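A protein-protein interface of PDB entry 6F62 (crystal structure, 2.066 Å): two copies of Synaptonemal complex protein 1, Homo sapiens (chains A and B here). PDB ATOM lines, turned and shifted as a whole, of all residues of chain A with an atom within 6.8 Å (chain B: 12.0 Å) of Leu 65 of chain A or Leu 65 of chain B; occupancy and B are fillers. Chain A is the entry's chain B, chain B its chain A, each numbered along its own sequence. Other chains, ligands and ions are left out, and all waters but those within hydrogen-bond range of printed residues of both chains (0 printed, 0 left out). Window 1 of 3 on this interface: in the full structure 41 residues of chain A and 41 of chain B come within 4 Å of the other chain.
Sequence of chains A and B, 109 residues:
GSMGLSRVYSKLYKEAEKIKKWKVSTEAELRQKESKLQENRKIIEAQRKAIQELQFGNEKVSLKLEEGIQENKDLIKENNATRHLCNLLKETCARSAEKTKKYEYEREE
Ser 62 of chain A touches one residue of chain B.
Of chain B, only Leu 65 comes within 4 Å of Lys 64 of chain A.
Of chain B, only Val 61, Lys 64 and Leu 65 come within 4 Å of Leu 65 of chain A.
No residue of chain B comes within 4 Å of Glu 66 of chain A.
Of chain B, only Asn 72 (3.2 Å) comes within 4 Å of Gly 68 of chain A.
No residue of chain B comes within 4 Å of Ile 69 of chain A.
Of the printed residues of chain A, Val 61 of chain B touches Val 61, Ser 62 and Leu 65.
Of the printed residues of chain A, Lys 64 of chain B touches Leu 65 (3.7 Å).
Printed residues of chain A within 4 Å of Asn 72 of chain B: Gly 68 (3.2 Å).
The nearest residue of chain A that does not touch Leu 65 of chain B is Gly 68 of chain A (5.9 Å).
The backbone carbonyl oxygen (O) of Asn 58 of chain B lies within hydrogen-bond range of the side-chain hydroxyl (OG) of Ser 62 of chain B (2.8 Å).
The side-chain amino group of Lys 64 of chain A is in salt-bridge range of the side-chain carboxylate of Glu 67 of chain A, at 2.8 Å.
The side-chain amide nitrogen (ND2) of Asn 72 of chain B is in hydrogen-bond range of the backbone carbonyl oxygen (O) of Gly 68 of chain A.
CG1 of Val 61 of chain A touches CG1 of Val 61 of chain B, at 3.7 Å.
Ser 62 of chain B touches Val 61 of chain A.
CG1 of Val 61 of chain A touches CD2 of Leu 65 of chain B, at 3.8 Å.
CG1 of Val 61 of chain B touches OG of Ser 62 of chain A, at 3.98 Å.
CD1 of Leu 65 of chain B touches C of Lys 64 of chain A (3.9 Å).
Val 61 of chain B touches Leu 65 of chain A.
O of Lys 64 of chain B touches CD1 of Leu 65 of chain A, at 3.7 Å.
N of Leu 65 of chain B touches CD1 of Leu 65 of chain A (3.7 Å).
Hydrophobic or aromatic side chains of chain B within 4 Å of the printed part of chain A: Val 61 and Leu 65.
Of the 11 printed residues of chain A, 5 touch a printed residue of chain B.
Hydrophobic or aromatic side chains of chain A that line the printed part of chain B: Val 61 and Leu 65.
Among the printed residues, 9 pairs touch across the chains.
Among the printed residues, no Asp or Glu carboxylate lies within 4 Å of a Lys or Arg side-chain nitrogen of the other chain.
Val 61 of chain B touches its own counterpart, Val 61 of chain A.
Val 61 of chain A touches Ser 62 of chain B, and with the chains exchanged Ser 62 of chain A touches Val 61 of chain B.
Val 61 of chain A touches Leu 65 of chain B, and with the chains exchanged Leu 65 of chain A touches Val 61 of chain B.
Leu 65 of chain A touches its own counterpart, Leu 65 of chain B.
Positions printed for both chains: 60, 61, 62, 63, 64, 65, 66, 67, 68, 69 and 70.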
ATOM      1  N   LYS A  60      -7.406 -22.719  -0.098  1.00  0.00           N
ATOM      2  CA  LYS A  60      -7.218 -23.188  -1.468  1.00  0.00           C
ATOM      3  C   LYS A  60      -8.515 -23.742  -2.043  1.00  0.00           C
ATOM      4  O   LYS A  60      -8.902 -23.404  -3.167  1.00  0.00           O
ATOM      5  CB  LYS A  60      -6.121 -24.252  -1.513  1.00  0.00           C
ATOM      6  CG  LYS A  60      -4.708 -23.700  -1.484  1.00  0.00           C
ATOM      7  CD  LYS A  60      -3.689 -24.823  -1.596  1.00  0.00           C
ATOM      8  CE  LYS A  60      -2.270 -24.293  -1.566  1.00  0.00           C
ATOM      9  NZ  LYS A  60      -1.276 -25.375  -1.315  1.00  0.00           N
ATOM     10  N   VAL A  61      -9.200 -24.603  -1.287  1.00  0.00           N
ATOM     11  CA  VAL A  61     -10.418 -25.223  -1.804  1.00  0.00           C
ATOM     12  C   VAL A  61     -11.479 -24.163  -2.071  1.00  0.00           C
ATOM     13  O   VAL A  61     -12.224 -24.244  -3.055  1.00  0.00           O
ATOM     14  CB  VAL A  61     -10.925 -26.304  -0.831  1.00  0.00           C
ATOM     15  CG1 VAL A  61     -12.165 -26.978  -1.390  1.00  0.00           C
ATOM     16  CG2 VAL A  61      -9.845 -27.344  -0.580  1.00  0.00           C
ATOM     17  N   SER A  62     -11.564 -23.151  -1.206  1.00  0.00           N
ATOM     18  CA  SER A  62     -12.523 -22.074  -1.432  1.00  0.00           C
ATOM     19  C   SER A  62     -12.227 -21.338  -2.732  1.00  0.00           C
ATOM     20  O   SER A  62     -13.145 -21.030  -3.502  1.00  0.00           O
ATOM     21  CB  SER A  62     -12.510 -21.104  -0.252  1.00  0.00           C
ATOM     22  OG  SER A  62     -12.949 -21.744   0.933  1.00  0.00           O
ATOM     23  N   LEU A  63     -10.950 -21.053  -2.998  1.00  0.00           N
ATOM     24  CA  LEU A  63     -10.591 -20.349  -4.225  1.00  0.00           C
ATOM     25  C   LEU A  63     -10.959 -21.168  -5.455  1.00  0.00           C
ATOM     26  O   LEU A  63     -11.531 -20.644  -6.417  1.00  0.00           O
ATOM     27  CB  LEU A  63      -9.098 -20.018  -4.219  1.00  0.00           C
ATOM     28  CG  LEU A  63      -8.649 -19.016  -3.153  1.00  0.00           C
ATOM     29  CD1 LEU A  63      -7.137 -18.859  -3.174  1.00  0.00           C
ATOM     30  CD2 LEU A  63      -9.324 -17.663  -3.347  1.00  0.00           C
ATOM     31  N   LYS A  64     -10.634 -22.463  -5.444  1.00  0.00           N
ATOM     32  CA  LYS A  64     -10.991 -23.310  -6.576  1.00  0.00           C
ATOM     33  C   LYS A  64     -12.502 -23.388  -6.749  1.00  0.00           C
ATOM     34  O   LYS A  64     -12.993 -23.482  -7.878  1.00  0.00           O
ATOM     35  CB  LYS A  64     -10.401 -24.708  -6.394  1.00  0.00           C
ATOM     36  CG  LYS A  64      -8.874 -24.752  -6.389  1.00  0.00           C
ATOM     37  CD  LYS A  64      -8.256 -24.177  -7.666  1.00  0.00           C
ATOM     38  CE  LYS A  64      -8.765 -24.882  -8.919  1.00  0.00           C
ATOM     39  NZ  LYS A  64      -8.092 -24.395 -10.155  1.00  0.00           N
ATOM     40  N   LEU A  65     -13.250 -23.344  -5.646  1.00  0.00           N
ATOM     41  CA  LEU A  65     -14.706 -23.341  -5.739  1.00  0.00           C
ATOM     42  C   LEU A  65     -15.206 -22.083  -6.440  1.00  0.00           C
ATOM     43  O   LEU A  65     -16.139 -22.142  -7.249  1.00  0.00           O
ATOM     44  CB  LEU A  65     -15.311 -23.467  -4.339  1.00  0.00           C
ATOM     45  CG  LEU A  65     -16.832 -23.560  -4.224  1.00  0.00           C
ATOM     46  CD1 LEU A  65     -17.365 -24.788  -4.946  1.00  0.00           C
ATOM     47  CD2 LEU A  65     -17.242 -23.580  -2.757  1.00  0.00           C
ATOM     48  N   GLU A  66     -14.588 -20.934  -6.150  1.00  0.00           N
ATOM     49  CA  GLU A  66     -14.971 -19.696  -6.824  1.00  0.00           C
ATOM     50  C   GLU A  66     -14.680 -19.768  -8.317  1.00  0.00           C
ATOM     51  O   GLU A  66     -15.484 -19.307  -9.137  1.00  0.00           O
ATOM     52  CB  GLU A  66     -14.239 -18.508  -6.199  1.00  0.00           C
ATOM     53  CG  GLU A  66     -14.592 -18.252  -4.746  1.00  0.00           C
ATOM     54  CD  GLU A  66     -13.706 -17.196  -4.107  1.00  0.00           C
ATOM     55  OE1 GLU A  66     -12.880 -16.594  -4.826  1.00  0.00           O
ATOM     56  OE2 GLU A  66     -13.837 -16.971  -2.885  1.00  0.00           O
ATOM     57  N   GLU A  67     -13.531 -20.334  -8.692  1.00  0.00           N
ATOM     58  CA  GLU A  67     -13.208 -20.477 -10.108  1.00  0.00           C
ATOM     59  C   GLU A  67     -14.230 -21.357 -10.816  1.00  0.00           C
ATOM     60  O   GLU A  67     -14.661 -21.046 -11.934  1.00  0.00           O
ATOM     61  CB  GLU A  67     -11.802 -21.055 -10.273  1.00  0.00           C
ATOM     62  CG  GLU A  67     -10.689 -20.139  -9.797  1.00  0.00           C
ATOM     63  CD  GLU A  67      -9.313 -20.736 -10.026  1.00  0.00           C
ATOM     64  OE1 GLU A  67      -9.236 -21.879 -10.526  1.00  0.00           O
ATOM     65  OE2 GLU A  67      -8.308 -20.065  -9.708  1.00  0.00           O
ATOM     66  N   GLY A  68     -14.634 -22.457 -10.180  1.00  0.00           N
ATOM     67  CA  GLY A  68     -15.599 -23.347 -10.802  1.00  0.00           C
ATOM     68  C   GLY A  68     -16.955 -22.694 -10.999  1.00  0.00           C
ATOM     69  O   GLY A  68     -17.595 -22.874 -12.039  1.00  0.00           O
ATOM     70  N   ILE A  69     -17.411 -21.929 -10.005  1.00  0.00           N
ATOM     71  CA  ILE A  69     -18.686 -21.226 -10.130  1.00  0.00           C
ATOM     72  C   ILE A  69     -18.665 -20.310 -11.345  1.00  0.00           C
ATOM     73  O   ILE A  69     -19.649 -20.214 -12.088  1.00  0.00           O
ATOM     74  CB  ILE A  69     -18.996 -20.450  -8.834  1.00  0.00           C
ATOM     75  CG1 ILE A  69     -19.351 -21.430  -7.713  1.00  0.00           C
ATOM     76  CG2 ILE A  69     -20.139 -19.449  -9.046  1.00  0.00           C
ATOM     77  CD1 ILE A  69     -19.433 -20.798  -6.340  1.00  0.00           C
ATOM     78  N   GLN A  70     -17.544 -19.628 -11.573  1.00  0.00           N
ATOM     79  CA  GLN A  70     -17.448 -18.735 -12.720  1.00  0.00           C
ATOM     80  C   GLN A  70     -17.428 -19.521 -14.025  1.00  0.00           C
ATOM     81  O   GLN A  70     -18.086 -19.137 -14.999  1.00  0.00           O
ATOM     82  CB  GLN A  70     -16.203 -17.860 -12.596  1.00  0.00           C
ATOM     83  CG  GLN A  70     -16.091 -16.796 -13.665  1.00  0.00           C
ATOM     84  CD  GLN A  70     -17.301 -15.881 -13.704  1.00  0.00           C
ATOM     85  OE1 GLN A  70     -17.641 -15.242 -12.708  1.00  0.00           O
ATOM     86  NE2 GLN A  70     -17.963 -15.822 -14.854  1.00  0.00           N
ATOM     87  N   PHE B  56     -14.266 -30.308   9.815  1.00  0.00           N
ATOM     88  CA  PHE B  56     -15.663 -30.308   9.394  1.00  0.00           C
ATOM     89  C   PHE B  56     -15.894 -29.312   8.265  1.00  0.00           C
ATOM     90  O   PHE B  56     -16.585 -29.621   7.286  1.00  0.00           O
ATOM     91  CB  PHE B  56     -16.563 -29.993  10.590  1.00  0.00           C
ATOM     92  CG  PHE B  56     -18.026 -30.208  10.325  1.00  0.00           C
ATOM     93  CD1 PHE B  56     -18.910 -29.143  10.349  1.00  0.00           C
ATOM     94  CD2 PHE B  56     -18.517 -31.475  10.054  1.00  0.00           C
ATOM     95  CE1 PHE B  56     -20.258 -29.337  10.110  1.00  0.00           C
ATOM     96  CE2 PHE B  56     -19.864 -31.674   9.811  1.00  0.00           C
ATOM     97  CZ  PHE B  56     -20.734 -30.603   9.838  1.00  0.00           C
ATOM     98  N   GLY B  57     -15.320 -28.113   8.379  1.00  0.00           N
ATOM     99  CA  GLY B  57     -15.444 -27.140   7.306  1.00  0.00           C
ATOM    100  C   GLY B  57     -14.793 -27.606   6.019  1.00  0.00           C
ATOM    101  O   GLY B  57     -15.345 -27.420   4.931  1.00  0.00           O
ATOM    102  N   ASN B  58     -13.608 -28.213   6.121  1.00  0.00           N
ATOM    103  CA  ASN B  58     -12.936 -28.723   4.929  1.00  0.00           C
ATOM    104  C   ASN B  58     -13.810 -29.727   4.191  1.00  0.00           C
ATOM    105  O   ASN B  58     -13.858 -29.729   2.955  1.00  0.00           O
ATOM    106  CB  ASN B  58     -11.598 -29.360   5.308  1.00  0.00           C
ATOM    107  CG  ASN B  58     -10.484 -28.341   5.451  1.00  0.00           C
ATOM    108  OD1 ASN B  58      -9.998 -27.795   4.462  1.00  0.00           O
ATOM    109  ND2 ASN B  58     -10.065 -28.089   6.684  1.00  0.00           N
ATOM    110  N   GLU B  59     -14.508 -30.594   4.928  1.00  0.00           N
ATOM    111  CA  GLU B  59     -15.385 -31.571   4.291  1.00  0.00           C
ATOM    112  C   GLU B  59     -16.504 -30.881   3.523  1.00  0.00           C
ATOM    113  O   GLU B  59     -16.809 -31.248   2.383  1.00  0.00           O
ATOM    114  CB  GLU B  59     -15.958 -32.526   5.339  1.00  0.00           C
ATOM    115  CG  GLU B  59     -15.050 -33.696   5.689  1.00  0.00           C
ATOM    116  CD  GLU B  59     -14.832 -34.637   4.521  1.00  0.00           C
ATOM    117  OE1 GLU B  59     -13.969 -34.341   3.668  1.00  0.00           O
ATOM    118  OE2 GLU B  59     -15.532 -35.669   4.449  1.00  0.00           O
ATOM    119  N   LYS B  60     -17.131 -29.874   4.136  1.00  0.00           N
ATOM    120  CA  LYS B  60     -18.194 -29.137   3.464  1.00  0.00           C
ATOM    121  C   LYS B  60     -17.715 -28.582   2.128  1.00  0.00           C
ATOM    122  O   LYS B  60     -18.271 -28.895   1.069  1.00  0.00           O
ATOM    123  CB  LYS B  60     -18.693 -27.997   4.353  1.00  0.00           C
ATOM    124  CG  LYS B  60     -19.720 -28.398   5.392  1.00  0.00           C
ATOM    125  CD  LYS B  60     -20.391 -27.165   5.977  1.00  0.00           C
ATOM    126  CE  LYS B  60     -21.158 -27.490   7.245  1.00  0.00           C
ATOM    127  NZ  LYS B  60     -21.806 -26.285   7.833  1.00  0.00           N
ATOM    128  N   VAL B  61     -16.670 -27.752   2.166  1.00  0.00           N
ATOM    129  CA  VAL B  61     -16.249 -27.041   0.963  1.00  0.00           C
ATOM    130  C   VAL B  61     -15.700 -28.011  -0.074  1.00  0.00           C
ATOM    131  O   VAL B  61     -15.866 -27.795  -1.280  1.00  0.00           O
ATOM    132  CB  VAL B  61     -15.219 -25.950   1.315  1.00  0.00           C
ATOM    133  CG1 VAL B  61     -14.937 -25.085   0.102  1.00  0.00           C
ATOM    134  CG2 VAL B  61     -15.714 -25.081   2.467  1.00  0.00           C
ATOM    135  N   SER B  62     -15.041 -29.089   0.363  1.00  0.00           N
ATOM    136  CA  SER B  62     -14.536 -30.076  -0.587  1.00  0.00           C
ATOM    137  C   SER B  62     -15.678 -30.740  -1.345  1.00  0.00           C
ATOM    138  O   SER B  62     -15.584 -30.957  -2.559  1.00  0.00           O
ATOM    139  CB  SER B  62     -13.693 -31.126   0.135  1.00  0.00           C
ATOM    140  OG  SER B  62     -12.511 -30.556   0.669  1.00  0.00           O
ATOM    141  N   LEU B  63     -16.767 -31.069  -0.646  1.00  0.00           N
ATOM    142  CA  LEU B  63     -17.926 -31.653  -1.314  1.00  0.00           C
ATOM    143  C   LEU B  63     -18.498 -30.692  -2.348  1.00  0.00           C
ATOM    144  O   LEU B  63     -18.800 -31.088  -3.481  1.00  0.00           O
ATOM    145  CB  LEU B  63     -18.991 -32.035  -0.285  1.00  0.00           C
ATOM    146  CG  LEU B  63     -18.675 -33.219   0.635  1.00  0.00           C
ATOM    147  CD1 LEU B  63     -19.805 -33.425   1.633  1.00  0.00           C
ATOM    148  CD2 LEU B  63     -18.430 -34.496  -0.155  1.00  0.00           C
ATOM    149  N   LYS B  64     -18.659 -29.419  -1.977  1.00  0.00           N
ATOM    150  CA  LYS B  64     -19.174 -28.435  -2.923  1.00  0.00           C
ATOM    151  C   LYS B  64     -18.272 -28.321  -4.146  1.00  0.00           C
ATOM    152  O   LYS B  64     -18.759 -28.193  -5.276  1.00  0.00           O
ATOM    153  CB  LYS B  64     -19.323 -27.073  -2.242  1.00  0.00           C
ATOM    154  CG  LYS B  64     -20.504 -26.978  -1.291  1.00  0.00           C
ATOM    155  CD  LYS B  64     -20.759 -25.537  -0.872  1.00  0.00           C
ATOM    156  CE  LYS B  64     -21.958 -25.432   0.060  1.00  0.00           C
ATOM    157  NZ  LYS B  64     -22.231 -24.024   0.465  1.00  0.00           N
ATOM    158  N   LEU B  65     -16.955 -28.365  -3.941  1.00  0.00           N
ATOM    159  CA  LEU B  65     -16.029 -28.284  -5.066  1.00  0.00           C
ATOM    160  C   LEU B  65     -16.215 -29.465  -6.010  1.00  0.00           C
ATOM    161  O   LEU B  65     -16.276 -29.294  -7.233  1.00  0.00           O
ATOM    162  CB  LEU B  65     -14.588 -28.224  -4.555  1.00  0.00           C
ATOM    163  CG  LEU B  65     -13.491 -28.232  -5.624  1.00  0.00           C
ATOM    164  CD1 LEU B  65     -13.666 -27.081  -6.602  1.00  0.00           C
ATOM    165  CD2 LEU B  65     -12.119 -28.170  -4.978  1.00  0.00           C
ATOM    166  N   GLU B  66     -16.311 -30.676  -5.457  1.00  0.00           N
ATOM    167  CA  GLU B  66     -16.444 -31.862  -6.296  1.00  0.00           C
ATOM    168  C   GLU B  66     -17.764 -31.859  -7.055  1.00  0.00           C
ATOM    169  O   GLU B  66     -17.814 -32.257  -8.226  1.00  0.00           O
ATOM    170  CB  GLU B  66     -16.314 -33.125  -5.444  1.00  0.00           C
ATOM    171  CG  GLU B  66     -14.949 -33.288  -4.787  1.00  0.00           C
ATOM    172  CD  GLU B  66     -13.821 -33.394  -5.795  1.00  0.00           C
ATOM    173  OE1 GLU B  66     -14.094 -33.742  -6.962  1.00  0.00           O
ATOM    174  OE2 GLU B  66     -12.659 -33.124  -5.421  1.00  0.00           O
ATOM    175  N   GLU B  67     -18.846 -31.414  -6.411  1.00  0.00           N
ATOM    176  CA  GLU B  67     -20.128 -31.326  -7.104  1.00  0.00           C
ATOM    177  C   GLU B  67     -20.055 -30.341  -8.264  1.00  0.00           C
ATOM    178  O   GLU B  67     -20.596 -30.603  -9.345  1.00  0.00           O
ATOM    179  CB  GLU B  67     -21.228 -30.917  -6.126  1.00  0.00           C
ATOM    180  CG  GLU B  67     -21.535 -31.961  -5.065  1.00  0.00           C
ATOM    181  CD  GLU B  67     -22.695 -31.561  -4.173  1.00  0.00           C
ATOM    182  OE1 GLU B  67     -23.345 -30.534  -4.465  1.00  0.00           O
ATOM    183  OE2 GLU B  67     -22.958 -32.273  -3.181  1.00  0.00           O
ATOM    184  N   GLY B  68     -19.393 -29.201  -8.058  1.00  0.00           N
ATOM    185  CA  GLY B  68     -19.260 -28.231  -9.133  1.00  0.00           C
ATOM    186  C   GLY B  68     -18.417 -28.747 -10.283  1.00  0.00           C
ATOM    187  O   GLY B  68     -18.754 -28.543 -11.452  1.00  0.00           O
ATOM    188  N   ILE B  69     -17.306 -29.421  -9.970  1.00  0.00           N
ATOM    189  CA  ILE B  69     -16.460 -29.997 -11.014  1.00  0.00           C
ATOM    190  C   ILE B  69     -17.276 -30.937 -11.891  1.00  0.00           C
ATOM    191  O   ILE B  69     -17.223 -30.869 -13.125  1.00  0.00           O
ATOM    192  CB  ILE B  69     -15.250 -30.715 -10.389  1.00  0.00           C
ATOM    193  CG1 ILE B  69     -14.279 -29.692  -9.799  1.00  0.00           C
ATOM    194  CG2 ILE B  69     -14.532 -31.592 -11.426  1.00  0.00           C
ATOM    195  CD1 ILE B  69     -13.149 -30.300  -8.992  1.00  0.00           C
ATOM    196  N   GLN B  70     -18.043 -31.831 -11.263  1.00  0.00           N
ATOM    197  CA  GLN B  70     -18.835 -32.785 -12.029  1.00  0.00           C
ATOM    198  C   GLN B  70     -19.901 -32.078 -12.854  1.00  0.00           C
ATOM    199  O   GLN B  70     -20.123 -32.424 -14.021  1.00  0.00           O
ATOM    200  CB  GLN B  70     -19.474 -33.808 -11.089  1.00  0.00           C
ATOM    201  CG  GLN B  70     -20.112 -34.986 -11.806  1.00  0.00           C
ATOM    202  CD  GLN B  70     -19.103 -35.802 -12.591  1.00  0.00           C
ATOM    203  OE1 GLN B  70     -19.195 -35.914 -13.813  1.00  0.00           O
ATOM    204  NE2 GLN B  70     -18.132 -36.374 -11.889  1.00  0.00           N
ATOM    205  N   GLU B  71     -20.571 -31.082 -12.268  1.00  0.00           N
ATOM    206  CA  GLU B  71     -21.589 -30.345 -13.006  1.00  0.00           C
ATOM    207  C   GLU B  71     -20.997 -29.668 -14.237  1.00  0.00           C
ATOM    208  O   GLU B  71     -21.616 -29.655 -15.307  1.00  0.00           O
ATOM    209  CB  GLU B  71     -22.250 -29.314 -12.090  1.00  0.00           C
ATOM    210  CG  GLU B  71     -23.402 -28.564 -12.734  1.00  0.00           C
ATOM    211  CD  GLU B  71     -24.133 -27.666 -11.755  1.00  0.00           C
ATOM    212  OE1 GLU B  71     -23.836 -27.738 -10.543  1.00  0.00           O
ATOM    213  OE2 GLU B  71     -25.004 -26.886 -12.197  1.00  0.00           O
ATOM    214  N   ASN B  72     -19.795 -29.102 -14.107  1.00  0.00           N
ATOM    215  CA  ASN B  72     -19.162 -28.447 -15.247  1.00  0.00           C
ATOM    216  C   ASN B  72     -18.756 -29.459 -16.313  1.00  0.00           C
ATOM    217  O   ASN B  72     -18.871 -29.184 -17.512  1.00  0.00           O
ATOM    218  CB  ASN B  72     -17.954 -27.636 -14.782  1.00  0.00           C
ATOM    219  CG  ASN B  72     -18.352 -26.361 -14.063  1.00  0.00           C
ATOM    220  OD1 ASN B  72     -19.479 -25.881 -14.199  1.00  0.00           O
ATOM    221  ND2 ASN B  72     -17.423 -25.798 -13.299  1.00  0.00           N
ATOM    222  N   LYS B  73     -18.275 -30.633 -15.898  1.00  0.00           N
ATOM    223  CA  LYS B  73     -17.956 -31.678 -16.868  1.00  0.00           C
ATOM    224  C   LYS B  73     -19.186 -32.072 -17.674  1.00  0.00           C
ATOM    225  O   LYS B  73     -19.090 -32.335 -18.880  1.00  0.00           O
ATOM    226  CB  LYS B  73     -17.368 -32.895 -16.154  1.00  0.00           C
ATOM    227  CG  LYS B  73     -15.928 -32.706 -15.699  1.00  0.00           C
ATOM    228  CD  LYS B  73     -15.424 -33.892 -14.883  1.00  0.00           C
ATOM    229  CE  LYS B  73     -13.953 -33.725 -14.514  1.00  0.00           C
ATOM    230  NZ  LYS B  73     -13.454 -34.816 -13.626  1.00  0.00           N
ATOM    231  N   ASP B  74     -20.354 -32.119 -17.030  1.00  0.00           N
ATOM    232  CA  ASP B  74     -21.577 -32.470 -17.744  1.00  0.00           C
ATOM    233  C   ASP B  74     -21.949 -31.400 -18.763  1.00  0.00           C
ATOM    234  O   ASP B  74     -22.370 -31.720 -19.880  1.00  0.00           O
ATOM    235  CB  ASP B  74     -22.722 -32.679 -16.753  1.00  0.00           C
ATOM    236  CG  ASP B  74     -22.482 -33.852 -15.824  1.00  0.00           C
ATOM    237  OD1 ASP B  74     -21.690 -34.749 -16.185  1.00  0.00           O
ATOM    238  OD2 ASP B  74     -23.091 -33.880 -14.733  1.00  0.00           O
ATOM    239  N   LEU B  75     -21.805 -30.125 -18.394  1.00  0.00           N
ATOM    240  CA  LEU B  75     -22.151 -29.048 -19.313  1.00  0.00           C
ATOM    241  C   LEU B  75     -21.278 -29.084 -20.561  1.00  0.00           C
ATOM    242  O   LEU B  75     -21.761 -28.840 -21.672  1.00  0.00           O
ATOM    243  CB  LEU B  75     -22.024 -27.700 -18.606  1.00  0.00           C
ATOM    244  CG  LEU B  75     -23.167 -27.363 -17.649  1.00  0.00           C
ATOM    245  CD1 LEU B  75     -22.766 -26.242 -16.707  1.00  0.00           C
ATOM    246  CD2 LEU B  75     -24.411 -26.984 -18.434  1.00  0.00           C
